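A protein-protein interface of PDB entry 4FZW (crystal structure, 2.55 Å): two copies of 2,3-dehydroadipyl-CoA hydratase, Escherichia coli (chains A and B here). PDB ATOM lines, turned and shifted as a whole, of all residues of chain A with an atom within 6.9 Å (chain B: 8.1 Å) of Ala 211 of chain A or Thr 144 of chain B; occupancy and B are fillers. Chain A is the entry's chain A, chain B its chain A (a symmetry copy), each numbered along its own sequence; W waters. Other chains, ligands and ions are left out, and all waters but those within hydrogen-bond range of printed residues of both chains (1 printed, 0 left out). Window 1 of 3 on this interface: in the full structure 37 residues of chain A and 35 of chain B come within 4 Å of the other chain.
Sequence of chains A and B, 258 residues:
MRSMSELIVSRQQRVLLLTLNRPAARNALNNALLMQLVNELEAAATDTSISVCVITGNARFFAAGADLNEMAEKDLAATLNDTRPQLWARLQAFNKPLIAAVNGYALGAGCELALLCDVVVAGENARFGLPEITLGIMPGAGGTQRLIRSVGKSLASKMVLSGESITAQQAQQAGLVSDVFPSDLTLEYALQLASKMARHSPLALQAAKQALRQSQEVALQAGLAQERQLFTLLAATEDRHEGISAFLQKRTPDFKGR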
ATOM      1  N   LEU A 205      15.504  26.782 -13.690  1.00  0.00           N
ATOM      2  CA  LEU A 205      15.699  27.946 -14.527  1.00  0.00           C
ATOM      3  C   LEU A 205      16.755  28.871 -13.948  1.00  0.00           C
ATOM      4  O   LEU A 205      17.689  29.266 -14.646  1.00  0.00           O
ATOM      5  CB  LEU A 205      14.379  28.690 -14.709  1.00  0.00           C
ATOM      6  CG  LEU A 205      13.361  27.870 -15.514  1.00  0.00           C
ATOM      7  CD1 LEU A 205      11.950  28.430 -15.376  1.00  0.00           C
ATOM      8  CD2 LEU A 205      13.779  27.756 -16.991  1.00  0.00           C
ATOM      9  N   GLN A 206      16.623  29.205 -12.667  1.00  0.00           N
ATOM     10  CA  GLN A 206      17.562  30.144 -12.034  1.00  0.00           C
ATOM     11  C   GLN A 206      18.996  29.612 -11.993  1.00  0.00           C
ATOM     12  O   GLN A 206      19.924  30.338 -12.315  1.00  0.00           O
ATOM     13  CB  GLN A 206      17.085  30.566 -10.649  1.00  0.00           C
ATOM     14  CG  GLN A 206      15.958  31.580 -10.660  1.00  0.00           C
ATOM     15  CD  GLN A 206      15.059  31.475  -9.440  1.00  0.00           C
ATOM     16  OE1 GLN A 206      14.976  30.435  -8.799  1.00  0.00           O
ATOM     17  NE2 GLN A 206      14.377  32.560  -9.122  1.00  0.00           N
ATOM     18  N   ALA A 207      19.163  28.339 -11.642  1.00  0.00           N
ATOM     19  CA  ALA A 207      20.488  27.710 -11.600  1.00  0.00           C
ATOM     20  C   ALA A 207      21.054  27.524 -13.006  1.00  0.00           C
ATOM     21  O   ALA A 207      22.233  27.784 -13.251  1.00  0.00           O
ATOM     22  CB  ALA A 207      20.416  26.370 -10.864  1.00  0.00           C
ATOM     23  N   ALA A 208      20.210  27.087 -13.937  1.00  0.00           N
ATOM     24  CA  ALA A 208      20.636  27.006 -15.329  1.00  0.00           C
ATOM     25  C   ALA A 208      21.064  28.385 -15.854  1.00  0.00           C
ATOM     26  O   ALA A 208      22.129  28.515 -16.470  1.00  0.00           O
ATOM     27  CB  ALA A 208      19.550  26.370 -16.219  1.00  0.00           C
ATOM     28  N   LYS A 209      20.266  29.418 -15.591  1.00  0.00           N
ATOM     29  CA  LYS A 209      20.642  30.745 -16.054  1.00  0.00           C
ATOM     30  C   LYS A 209      21.923  31.265 -15.395  1.00  0.00           C
ATOM     31  O   LYS A 209      22.718  31.965 -16.029  1.00  0.00           O
ATOM     32  CB  LYS A 209      19.524  31.766 -15.859  1.00  0.00           C
ATOM     33  CG  LYS A 209      20.001  33.161 -16.246  1.00  0.00           C
ATOM     34  CD  LYS A 209      18.995  34.246 -15.988  1.00  0.00           C
ATOM     35  CE  LYS A 209      19.589  35.598 -16.348  1.00  0.00           C
ATOM     36  NZ  LYS A 209      18.526  36.611 -16.330  1.00  0.00           N
ATOM     37  N   GLN A 210      22.108  30.944 -14.117  1.00  0.00           N
ATOM     38  CA  GLN A 210      23.309  31.371 -13.406  1.00  0.00           C
ATOM     39  C   GLN A 210      24.526  30.677 -14.014  1.00  0.00           C
ATOM     40  O   GLN A 210      25.532  31.324 -14.285  1.00  0.00           O
ATOM     41  CB  GLN A 210      23.204  31.070 -11.915  1.00  0.00           C
ATOM     42  CG  GLN A 210      24.373  31.575 -11.075  1.00  0.00           C
ATOM     43  CD  GLN A 210      24.533  33.082 -11.149  1.00  0.00           C
ATOM     44  OE1 GLN A 210      23.640  33.807 -11.610  1.00  0.00           O
ATOM     45  NE2 GLN A 210      25.675  33.565 -10.691  1.00  0.00           N
ATOM     46  N   ALA A 211      24.413  29.368 -14.251  1.00  0.00           N
ATOM     47  CA  ALA A 211      25.418  28.614 -15.000  1.00  0.00           C
ATOM     48  C   ALA A 211      25.810  29.355 -16.265  1.00  0.00           C
ATOM     49  O   ALA A 211      26.999  29.483 -16.580  1.00  0.00           O
ATOM     50  CB  ALA A 211      24.893  27.217 -15.364  1.00  0.00           C
ATOM     51  N   LEU A 212      24.799  29.831 -16.989  1.00  0.00           N
ATOM     52  CA  LEU A 212      25.012  30.488 -18.276  1.00  0.00           C
ATOM     53  C   LEU A 212      25.717  31.829 -18.149  1.00  0.00           C
ATOM     54  O   LEU A 212      26.644  32.110 -18.918  1.00  0.00           O
ATOM     55  CB  LEU A 212      23.697  30.635 -19.065  1.00  0.00           C
ATOM     56  CG  LEU A 212      23.147  29.377 -19.729  1.00  0.00           C
ATOM     57  CD1 LEU A 212      21.626  29.429 -19.752  1.00  0.00           C
ATOM     58  CD2 LEU A 212      23.731  29.219 -21.126  1.00  0.00           C
ATOM     59  N   ARG A 213      25.278  32.647 -17.187  1.00  0.00           N
ATOM     60  CA  ARG A 213      25.929  33.931 -16.904  1.00  0.00           C
ATOM     61  C   ARG A 213      27.399  33.745 -16.634  1.00  0.00           C
ATOM     62  O   ARG A 213      28.242  34.464 -17.175  1.00  0.00           O
ATOM     63  CB  ARG A 213      25.293  34.613 -15.707  1.00  0.00           C
ATOM     64  CG  ARG A 213      23.910  35.155 -16.001  1.00  0.00           C
ATOM     65  CD  ARG A 213      23.958  36.601 -16.482  1.00  0.00           C
ATOM     66  NE  ARG A 213      24.126  37.530 -15.363  1.00  0.00           N
ATOM     67  CZ  ARG A 213      25.283  38.074 -15.000  1.00  0.00           C
ATOM     68  NH1 ARG A 213      25.321  38.908 -13.973  1.00  0.00           N
ATOM     69  NH2 ARG A 213      26.399  37.789 -15.666  1.00  0.00           N
ATOM     70  N   GLN A 214      27.692  32.743 -15.812  1.00  0.00           N
ATOM     71  CA  GLN A 214      29.048  32.522 -15.333  1.00  0.00           C
ATOM     72  C   GLN A 214      30.009  32.047 -16.427  1.00  0.00           C
ATOM     73  O   GLN A 214      31.207  32.316 -16.347  1.00  0.00           O
ATOM     74  CB  GLN A 214      29.043  31.620 -14.105  1.00  0.00           C
ATOM     75  CG  GLN A 214      28.361  32.300 -12.908  1.00  0.00           C
ATOM     76  CD  GLN A 214      29.032  33.640 -12.510  1.00  0.00           C
ATOM     77  OE1 GLN A 214      28.438  34.721 -12.635  1.00  0.00           O
ATOM     78  NE2 GLN A 214      30.263  33.555 -12.008  1.00  0.00           N
ATOM     79  N   SER A 215      29.481  31.396 -17.463  1.00  0.00           N
ATOM     80  CA  SER A 215      30.297  31.022 -18.603  1.00  0.00           C
ATOM     81  C   SER A 215      30.986  32.247 -19.207  1.00  0.00           C
ATOM     82  O   SER A 215      32.081  32.118 -19.771  1.00  0.00           O
ATOM     83  CB  SER A 215      29.493  30.263 -19.681  1.00  0.00           C
ATOM     84  OG  SER A 215      28.554  31.096 -20.342  1.00  0.00           O
ATOM     85  N   GLN A 216      30.364  33.425 -19.102  1.00  0.00           N
ATOM     86  CA  GLN A 216      30.967  34.641 -19.666  1.00  0.00           C
ATOM     87  C   GLN A 216      31.978  35.246 -18.677  1.00  0.00           C
ATOM     88  O   GLN A 216      32.719  36.196 -18.982  1.00  0.00           O
ATOM     89  CB  GLN A 216      29.913  35.690 -20.027  1.00  0.00           C
ATOM     90  CG  GLN A 216      28.727  35.179 -20.801  1.00  0.00           C
ATOM     91  CD  GLN A 216      29.081  34.773 -22.217  1.00  0.00           C
ATOM     92  OE1 GLN A 216      28.964  35.565 -23.159  1.00  0.00           O
ATOM     93  NE2 GLN A 216      29.529  33.531 -22.373  1.00  0.00           N
ATOM     94  N   GLY A 223      34.240  26.976 -15.211  1.00  0.00           N
ATOM     95  CA  GLY A 223      32.842  26.979 -15.595  1.00  0.00           C
ATOM     96  C   GLY A 223      32.220  25.617 -15.322  1.00  0.00           C
ATOM     97  O   GLY A 223      31.103  25.532 -14.810  1.00  0.00           O
ATOM     98  N   LEU A 224      32.943  24.553 -15.681  1.00  0.00           N
ATOM     99  CA  LEU A 224      32.502  23.183 -15.446  1.00  0.00           C
ATOM    100  C   LEU A 224      32.299  22.895 -13.962  1.00  0.00           C
ATOM    101  O   LEU A 224      31.303  22.274 -13.580  1.00  0.00           O
ATOM    102  CB  LEU A 224      33.517  22.194 -16.021  1.00  0.00           C
ATOM    103  CG  LEU A 224      33.637  22.232 -17.535  1.00  0.00           C
ATOM    104  CD1 LEU A 224      34.737  21.314 -18.021  1.00  0.00           C
ATOM    105  CD2 LEU A 224      32.319  21.793 -18.096  1.00  0.00           C
ATOM    106  N   GLN A 226      31.712  25.013 -11.515  1.00  0.00           N
ATOM    107  CA  GLN A 226      30.629  25.872 -11.070  1.00  0.00           C
ATOM    108  C   GLN A 226      29.285  25.301 -11.515  1.00  0.00           C
ATOM    109  O   GLN A 226      28.284  25.394 -10.798  1.00  0.00           O
ATOM    110  CB  GLN A 226      30.856  27.258 -11.685  1.00  0.00           C
ATOM    111  CG  GLN A 226      29.822  28.314 -11.386  1.00  0.00           C
ATOM    112  CD  GLN A 226      30.455  29.616 -10.883  1.00  0.00           C
ATOM    113  OE1 GLN A 226      31.005  29.658  -9.801  1.00  0.00           O
ATOM    114  NE2 GLN A 226      30.396  30.664 -11.679  1.00  0.00           N
ATOM    115  N   GLU A 227      29.268  24.712 -12.708  1.00  0.00           N
ATOM    116  CA  GLU A 227      28.070  24.058 -13.233  1.00  0.00           C
ATOM    117  C   GLU A 227      27.769  22.814 -12.399  1.00  0.00           C
ATOM    118  O   GLU A 227      26.644  22.572 -11.987  1.00  0.00           O
ATOM    119  CB  GLU A 227      28.291  23.650 -14.687  1.00  0.00           C
ATOM    120  CG  GLU A 227      27.181  22.791 -15.262  1.00  0.00           C
ATOM    121  CD  GLU A 227      27.564  22.129 -16.578  1.00  0.00           C
ATOM    122  OE1 GLU A 227      28.076  20.991 -16.537  1.00  0.00           O
ATOM    123  OE2 GLU A 227      27.347  22.747 -17.642  1.00  0.00           O
ATOM    124  N   ARG A 228      28.797  22.027 -12.137  1.00  0.00           N
ATOM    125  CA  ARG A 228      28.669  20.957 -11.168  1.00  0.00           C
ATOM    126  C   ARG A 228      28.034  21.415  -9.848  1.00  0.00           C
ATOM    127  O   ARG A 228      27.077  20.787  -9.394  1.00  0.00           O
ATOM    128  CB  ARG A 228      30.008  20.225 -10.981  1.00  0.00           C
ATOM    129  CG  ARG A 228      30.336  19.333 -12.202  1.00  0.00           C
ATOM    130  CD  ARG A 228      29.108  18.501 -12.567  1.00  0.00           C
ATOM    131  NE  ARG A 228      28.743  17.636 -11.443  1.00  0.00           N
ATOM    132  CZ  ARG A 228      27.737  16.764 -11.431  1.00  0.00           C
ATOM    133  NH1 ARG A 228      26.950  16.619 -12.493  1.00  0.00           N
ATOM    134  NH2 ARG A 228      27.515  16.030 -10.343  1.00  0.00           N
ATOM    135  N   LEU A 230      26.126  24.134  -9.135  1.00  0.00           N
ATOM    136  CA  LEU A 230      24.709  24.506  -9.355  1.00  0.00           C
ATOM    137  C   LEU A 230      23.871  23.256  -9.681  1.00  0.00           C
ATOM    138  O   LEU A 230      22.720  23.139  -9.273  1.00  0.00           O
ATOM    139  CB  LEU A 230      24.573  25.567 -10.446  1.00  0.00           C
ATOM    140  CG  LEU A 230      25.015  27.013 -10.116  1.00  0.00           C
ATOM    141  CD1 LEU A 230      25.488  27.747 -11.352  1.00  0.00           C
ATOM    142  CD2 LEU A 230      23.945  27.850  -9.405  1.00  0.00           C
ATOM    143  N   GLU B 112      26.122  16.567 -24.688  1.00  0.00           N
ATOM    144  CA  GLU B 112      27.258  17.058 -23.922  1.00  0.00           C
ATOM    145  C   GLU B 112      28.489  16.267 -24.305  1.00  0.00           C
ATOM    146  O   GLU B 112      29.596  16.789 -24.289  1.00  0.00           O
ATOM    147  CB  GLU B 112      26.998  16.953 -22.431  1.00  0.00           C
ATOM    148  CG  GLU B 112      25.843  17.817 -21.959  1.00  0.00           C
ATOM    149  CD  GLU B 112      25.552  17.643 -20.486  1.00  0.00           C
ATOM    150  OE1 GLU B 112      25.011  16.586 -20.087  1.00  0.00           O
ATOM    151  OE2 GLU B 112      25.860  18.584 -19.732  1.00  0.00           O
ATOM    152  N   LEU B 115      29.650  17.840 -27.719  1.00  0.00           N
ATOM    153  CA  LEU B 115      30.302  19.110 -27.383  1.00  0.00           C
ATOM    154  C   LEU B 115      31.698  18.916 -26.767  1.00  0.00           C
ATOM    155  O   LEU B 115      32.591  19.742 -26.951  1.00  0.00           O
ATOM    156  CB  LEU B 115      29.433  19.907 -26.412  1.00  0.00           C
ATOM    157  CG  LEU B 115      28.147  20.518 -26.968  1.00  0.00           C
ATOM    158  CD1 LEU B 115      27.208  20.973 -25.847  1.00  0.00           C
ATOM    159  CD2 LEU B 115      28.510  21.673 -27.886  1.00  0.00           C
ATOM    160  N   LEU B 130      19.414  19.751 -25.194  1.00  0.00           N
ATOM    161  CA  LEU B 130      19.594  19.608 -23.776  1.00  0.00           C
ATOM    162  C   LEU B 130      18.237  19.668 -23.083  1.00  0.00           C
ATOM    163  O   LEU B 130      17.770  20.747 -22.705  1.00  0.00           O
ATOM    164  CB  LEU B 130      20.532  20.705 -23.265  1.00  0.00           C
ATOM    165  CG  LEU B 130      21.958  20.586 -23.822  1.00  0.00           C
ATOM    166  CD1 LEU B 130      22.705  21.907 -23.703  1.00  0.00           C
ATOM    167  CD2 LEU B 130      22.742  19.418 -23.188  1.00  0.00           C
ATOM    168  N   GLU B 132      17.575  18.605 -20.157  1.00  0.00           N
ATOM    169  CA  GLU B 132      17.709  18.502 -18.694  1.00  0.00           C
ATOM    170  C   GLU B 132      16.667  19.358 -17.994  1.00  0.00           C
ATOM    171  O   GLU B 132      15.957  18.899 -17.113  1.00  0.00           O
ATOM    172  CB  GLU B 132      19.109  18.873 -18.218  1.00  0.00           C
ATOM    173  CG  GLU B 132      20.169  17.798 -18.492  1.00  0.00           C
ATOM    174  CD  GLU B 132      20.699  17.847 -19.913  1.00  0.00           C
ATOM    175  OE1 GLU B 132      20.233  18.715 -20.680  1.00  0.00           O
ATOM    176  OE2 GLU B 132      21.592  17.038 -20.259  1.00  0.00           O
ATOM    177  N   MET B 138      19.265  20.208 -15.025  1.00  0.00           N
ATOM    178  CA  MET B 138      19.950  21.102 -15.943  1.00  0.00           C
ATOM    179  C   MET B 138      21.167  20.339 -16.419  1.00  0.00           C
ATOM    180  O   MET B 138      21.437  19.256 -15.919  1.00  0.00           O
ATOM    181  CB  MET B 138      20.390  22.352 -15.199  1.00  0.00           C
ATOM    182  CG  MET B 138      21.296  22.013 -14.005  1.00  0.00           C
ATOM    183  SD  MET B 138      21.957  23.440 -13.132  1.00  0.00           S
ATOM    184  CE  MET B 138      23.214  23.993 -14.263  1.00  0.00           C
ATOM    185  N   PRO B 139      21.922  20.898 -17.372  1.00  0.00           N
ATOM    186  CA  PRO B 139      23.106  20.161 -17.818  1.00  0.00           C
ATOM    187  C   PRO B 139      24.182  20.087 -16.724  1.00  0.00           C
ATOM    188  O   PRO B 139      24.531  21.096 -16.145  1.00  0.00           O
ATOM    189  CB  PRO B 139      23.600  20.978 -19.030  1.00  0.00           C
ATOM    190  CG  PRO B 139      22.488  21.916 -19.355  1.00  0.00           C
ATOM    191  CD  PRO B 139      21.757  22.169 -18.097  1.00  0.00           C
ATOM    192  N   GLY B 140      24.705  18.896 -16.463  1.00  0.00           N
ATOM    193  CA  GLY B 140      25.758  18.711 -15.476  1.00  0.00           C
ATOM    194  C   GLY B 140      27.045  18.118 -16.033  1.00  0.00           C
ATOM    195  O   GLY B 140      27.805  17.490 -15.312  1.00  0.00           O
ATOM    196  N   ALA B 141      27.279  18.298 -17.329  1.00  0.00           N
ATOM    197  CA  ALA B 141      28.468  17.743 -17.971  1.00  0.00           C
ATOM    198  C   ALA B 141      28.983  18.669 -19.070  1.00  0.00           C
ATOM    199  O   ALA B 141      29.462  18.219 -20.106  1.00  0.00           O
ATOM    200  CB  ALA B 141      28.215  16.282 -18.502  1.00  0.00           C
ATOM    201  N   GLY B 142      28.871  19.969 -18.844  1.00  0.00           N
ATOM    202  CA  GLY B 142      29.473  20.926 -19.754  1.00  0.00           C
ATOM    203  C   GLY B 142      28.485  21.587 -20.695  1.00  0.00           C
ATOM    204  O   GLY B 142      28.845  22.510 -21.442  1.00  0.00           O
ATOM    205  N   GLY B 143      27.241  21.117 -20.663  1.00  0.00           N
ATOM    206  CA  GLY B 143      26.203  21.683 -21.495  1.00  0.00           C
ATOM    207  C   GLY B 143      26.093  23.195 -21.390  1.00  0.00           C
ATOM    208  O   GLY B 143      26.060  23.891 -22.400  1.00  0.00           O
ATOM    209  N   THR B 144      26.041  23.709 -20.165  1.00  0.00           N
ATOM    210  CA  THR B 144      25.931  25.157 -19.927  1.00  0.00           C
ATOM    211  C   THR B 144      27.201  25.981 -20.190  1.00  0.00           C
ATOM    212  O   THR B 144      27.156  27.206 -20.109  1.00  0.00           O
ATOM    213  CB  THR B 144      25.428  25.460 -18.497  1.00  0.00           C
ATOM    214  OG1 THR B 144      26.437  25.118 -17.527  1.00  0.00           O
ATOM    215  CG2 THR B 144      24.156  24.681 -18.215  1.00  0.00           C
ATOM    216  N   GLN B 145      28.311  25.328 -20.526  1.00  0.00           N
ATOM    217  CA  GLN B 145      29.551  26.050 -20.808  1.00  0.00           C
ATOM    218  C   GLN B 145      29.995  25.920 -22.259  1.00  0.00           C
ATOM    219  O   GLN B 145      30.302  26.916 -22.919  1.00  0.00           O
ATOM    220  CB  GLN B 145      30.685  25.580 -19.884  1.00  0.00           C
ATOM    221  CG  GLN B 145      30.347  25.651 -18.403  1.00  0.00           C
ATOM    222  CD  GLN B 145      30.009  27.064 -17.957  1.00  0.00           C
ATOM    223  OE1 GLN B 145      30.828  27.980 -18.079  1.00  0.00           O
ATOM    224  NE2 GLN B 145      28.799  27.245 -17.424  1.00  0.00           N
ATOM    225  N   ARG B 146      30.018  24.692 -22.761  1.00  0.00           N
ATOM    226  CA  ARG B 146      30.534  24.443 -24.098  1.00  0.00           C
ATOM    227  C   ARG B 146      29.621  24.904 -25.240  1.00  0.00           C
ATOM    228  O   ARG B 146      30.102  25.403 -26.258  1.00  0.00           O
ATOM    229  CB  ARG B 146      30.891  22.974 -24.255  1.00  0.00           C
ATOM    230  CG  ARG B 146      32.228  22.642 -23.702  1.00  0.00           C
ATOM    231  CD  ARG B 146      32.553  21.191 -23.911  1.00  0.00           C
ATOM    232  NE  ARG B 146      32.252  20.426 -22.716  1.00  0.00           N
ATOM    233  CZ  ARG B 146      33.172  19.845 -21.958  1.00  0.00           C
ATOM    234  NH1 ARG B 146      34.452  19.922 -22.292  1.00  0.00           N
ATOM    235  NH2 ARG B 146      32.806  19.169 -20.878  1.00  0.00           N
ATOM    236  N   LEU B 147      28.311  24.729 -25.084  1.00  0.00           N
ATOM    237  CA  LEU B 147      27.380  25.128 -26.130  1.00  0.00           C
ATOM    238  C   LEU B 147      27.501  26.622 -26.400  1.00  0.00           C
ATOM    239  O   LEU B 147      27.808  27.032 -27.524  1.00  0.00           O
ATOM    240  CB  LEU B 147      25.946  24.758 -25.750  1.00  0.00           C
ATOM    241  CG  LEU B 147      24.845  25.131 -26.755  1.00  0.00           C
ATOM    242  CD1 LEU B 147      25.142  24.580 -28.153  1.00  0.00           C
ATOM    243  CD2 LEU B 147      23.499  24.631 -26.275  1.00  0.00           C
ATOM    244  N   ILE B 148      27.285  27.416 -25.351  1.00  0.00           N
ATOM    245  CA  ILE B 148      27.287  28.875 -25.449  1.00  0.00           C
ATOM    246  C   ILE B 148      28.582  29.411 -26.049  1.00  0.00           C
ATOM    247  O   ILE B 148      28.579  30.470 -26.682  1.00  0.00           O
ATOM    248  CB  ILE B 148      27.019  29.558 -24.078  1.00  0.00           C
ATOM    249  CG1 ILE B 148      26.747  31.054 -24.260  1.00  0.00           C
ATOM    250  CG2 ILE B 148      28.191  29.320 -23.089  1.00  0.00           C
ATOM    251  CD1 ILE B 148      26.242  31.746 -23.007  1.00  0.00           C
ATOM    252  N   ARG B 149      29.688  28.693 -25.862  1.00  0.00           N
ATOM    253  CA  ARG B 149      30.953  29.138 -26.451  1.00  0.00           C
ATOM    254  C   ARG B 149      31.024  28.981 -27.992  1.00  0.00           C
ATOM    255  O   ARG B 149      31.700  29.755 -28.687  1.00  0.00           O
ATOM    256  CB  ARG B 149      32.161  28.483 -25.748  1.00  0.00           C
ATOM    257  CG  ARG B 149      32.426  29.039 -24.356  1.00  0.00           C
ATOM    258  CD  ARG B 149      33.557  28.276 -23.651  1.00  0.00           C
ATOM    259  NE  ARG B 149      34.034  28.966 -22.459  1.00  0.00           N
ATOM    260  CZ  ARG B 149      33.373  28.990 -21.307  1.00  0.00           C
ATOM    261  NH1 ARG B 149      32.210  28.352 -21.208  1.00  0.00           N
ATOM    262  NH2 ARG B 149      33.868  29.636 -20.257  1.00  0.00           N
ATOM    263  N   ALA B 156      22.079  29.163 -27.215  1.00  0.00           N
ATOM    264  CA  ALA B 156      22.430  28.261 -26.129  1.00  0.00           C
ATOM    265  C   ALA B 156      21.477  28.439 -24.961  1.00  0.00           C
ATOM    266  O   ALA B 156      21.136  27.474 -24.274  1.00  0.00           O
ATOM    267  CB  ALA B 156      23.848  28.490 -25.671  1.00  0.00           C
ATOM    268  N   SER B 157      21.039  29.671 -24.725  1.00  0.00           N
ATOM    269  CA  SER B 157      20.136  29.917 -23.608  1.00  0.00           C
ATOM    270  C   SER B 157      18.750  29.337 -23.877  1.00  0.00           C
ATOM    271  O   SER B 157      18.176  28.655 -23.028  1.00  0.00           O
ATOM    272  CB  SER B 157      20.099  31.405 -23.262  1.00  0.00           C
ATOM    273  OG  SER B 157      21.376  31.795 -22.799  1.00  0.00           O
ATOM    274  N   VAL B 160      19.102  25.617 -23.527  1.00  0.00           N
ATOM    275  CA  VAL B 160      19.292  25.214 -22.150  1.00  0.00           C
ATOM    276  C   VAL B 160      18.070  25.525 -21.288  1.00  0.00           C
ATOM    277  O   VAL B 160      17.667  24.684 -20.474  1.00  0.00           O
ATOM    278  CB  VAL B 160      20.551  25.868 -21.550  1.00  0.00           C
ATOM    279  CG1 VAL B 160      20.519  25.880 -19.993  1.00  0.00           C
ATOM    280  CG2 VAL B 160      21.805  25.200 -22.107  1.00  0.00           C
ATOM    281  N   LEU B 161      17.464  26.701 -21.483  1.00  0.00           N
ATOM    282  CA  LEU B 161      16.301  27.105 -20.677  1.00  0.00           C
ATOM    283  C   LEU B 161      14.927  26.519 -21.102  1.00  0.00           C
ATOM    284  O   LEU B 161      14.036  26.326 -20.265  1.00  0.00           O
ATOM    285  CB  LEU B 161      16.217  28.637 -20.581  1.00  0.00           C
ATOM    286  CG  LEU B 161      17.322  29.476 -19.939  1.00  0.00           C
ATOM    287  CD1 LEU B 161      17.133  30.946 -20.283  1.00  0.00           C
ATOM    288  CD2 LEU B 161      17.447  29.256 -18.390  1.00  0.00           C
HETATM  289  O   HOH W   1      30.798  32.110 -25.127  1.00  0.00           O
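O of Ala 211 of chain A sits at hydrogen-bond distance from NE2 of Gln 145 of chain B, 3.0 Å away.
O of Ser 215 of chain A is in hydrogen-bond range of NH2 of Arg 149 of chain B.
N of Ala 141 of chain B sits at hydrogen-bond distance from OE1 of Glu 227 of chain A (2.9 Å).
The side-chain carboxylate (OE1) of Glu 227 of chain A sits at hydrogen-bond distance from the backbone NH (N) of Gly 142 of chain B, 2.6 Å away.
OE2 of Glu 227 of chain A is in hydrogen-bond range of N of Gly 143 of chain B (3.4 Å).
The side-chain hydroxyl (OG1) of Thr 144 of chain B is in hydrogen-bond range of the side-chain carboxylate (OE2) of Glu 227 of chain A.
The guanidinium group (NH1) of Arg 228 of chain A lies within hydrogen-bond range of the backbone carbonyl oxygen (O) of Gly 140 of chain B.
OG of Ser 215 of chain A lies within hydrogen-bond range of O of Leu 212 of chain A.
NE2 of Gln 216 of chain A lies within hydrogen-bond range of OG of Ser 215 of chain A (3.3 Å).
The side-chain carboxylate of Glu 112 of chain B sits at hydrogen-bond distance from the backbone NH of Ala 141 of chain B, at 2.8 Å.
The side-chain carboxylate (OE2) of Glu 112 of chain B lies within hydrogen-bond range of the backbone NH (N) of Gly 142 of chain B.
The side-chain hydroxyl (OG1) of Thr 144 of chain B is in hydrogen-bond range of the side-chain amide nitrogen (NE2) of Gln 145 of chain B (3.2 Å).
The backbone carbonyl oxygen (O) of Gln 145 of chain B is in hydrogen-bond range of the guanidinium group (NH1) of Arg 149 of chain B, at 2.9 Å.
Leu 205 of chain A touches Leu 161 of chain B.
Ala 208 of chain A touches Val 160 of chain B (CB to CG1, 3.9 Å).
Lys 209 of chain A touches Leu 161 of chain B (N to CD2, 3.98 Å).
OG1 of Thr 144 of chain B touches CB of Ala 211 of chain A, 3.4 Å away.
Leu 212 of chain A touches Val 160 of chain B.
Ser 215 of chain A touches Thr 144 of chain B.
Gly 223 of chain A touches Gln 145 of chain B (CA to OE1, 3.4 Å).
Leu 224 of chain A touches Gly 142 of chain B (CD2 to CA, 3.4 Å).
OE1 of Glu 227 of chain A touches C of Gly 140 of chain B, 3.1 Å away.
Met 138 of chain B touches Leu 230 of chain A (SD to O, 3.9 Å).
Thr 144 of chain B touches just these residues of chain A: Ala 211, Ser 215 and Glu 227.
Of the printed residues of chain A, Arg 149 of chain B touches Ser 215.
Of the printed residues of chain A, Gln 145 of chain B touches Ala 211, Ser 215, Gly 223, Leu 224 and Glu 227.
Gln 206 of chain A touches none of the printed residues of chain B.
Leu 147 of chain B touches none of the printed residues of chain A.
The nearest residue of chain B that does not touch Ala 211 of chain A is Pro 139 of chain B (6.2 Å).
Hydrophobic or aromatic side chains of chain A that line the printed part of chain B: Leu 205, Ala 208, Ala 211, Leu 212 and Leu 224.
Along chain A the printed residues that touch a printed residue of chain B span positions 205 to 230.
Along chain B the printed residues that touch a printed residue of chain A span positions 138 to 161.
Among the printed residues, no Asp or Glu carboxylate lies within 4 Å of a Lys or Arg side-chain nitrogen of the other chain.
No position is printed for both chains.
Water W1 bridges the backbone carbonyl oxygen of Ile 148 of chain B (3.2 Å) and the side-chain amide nitrogen of Gln 216 of chain A (3.3 Å).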
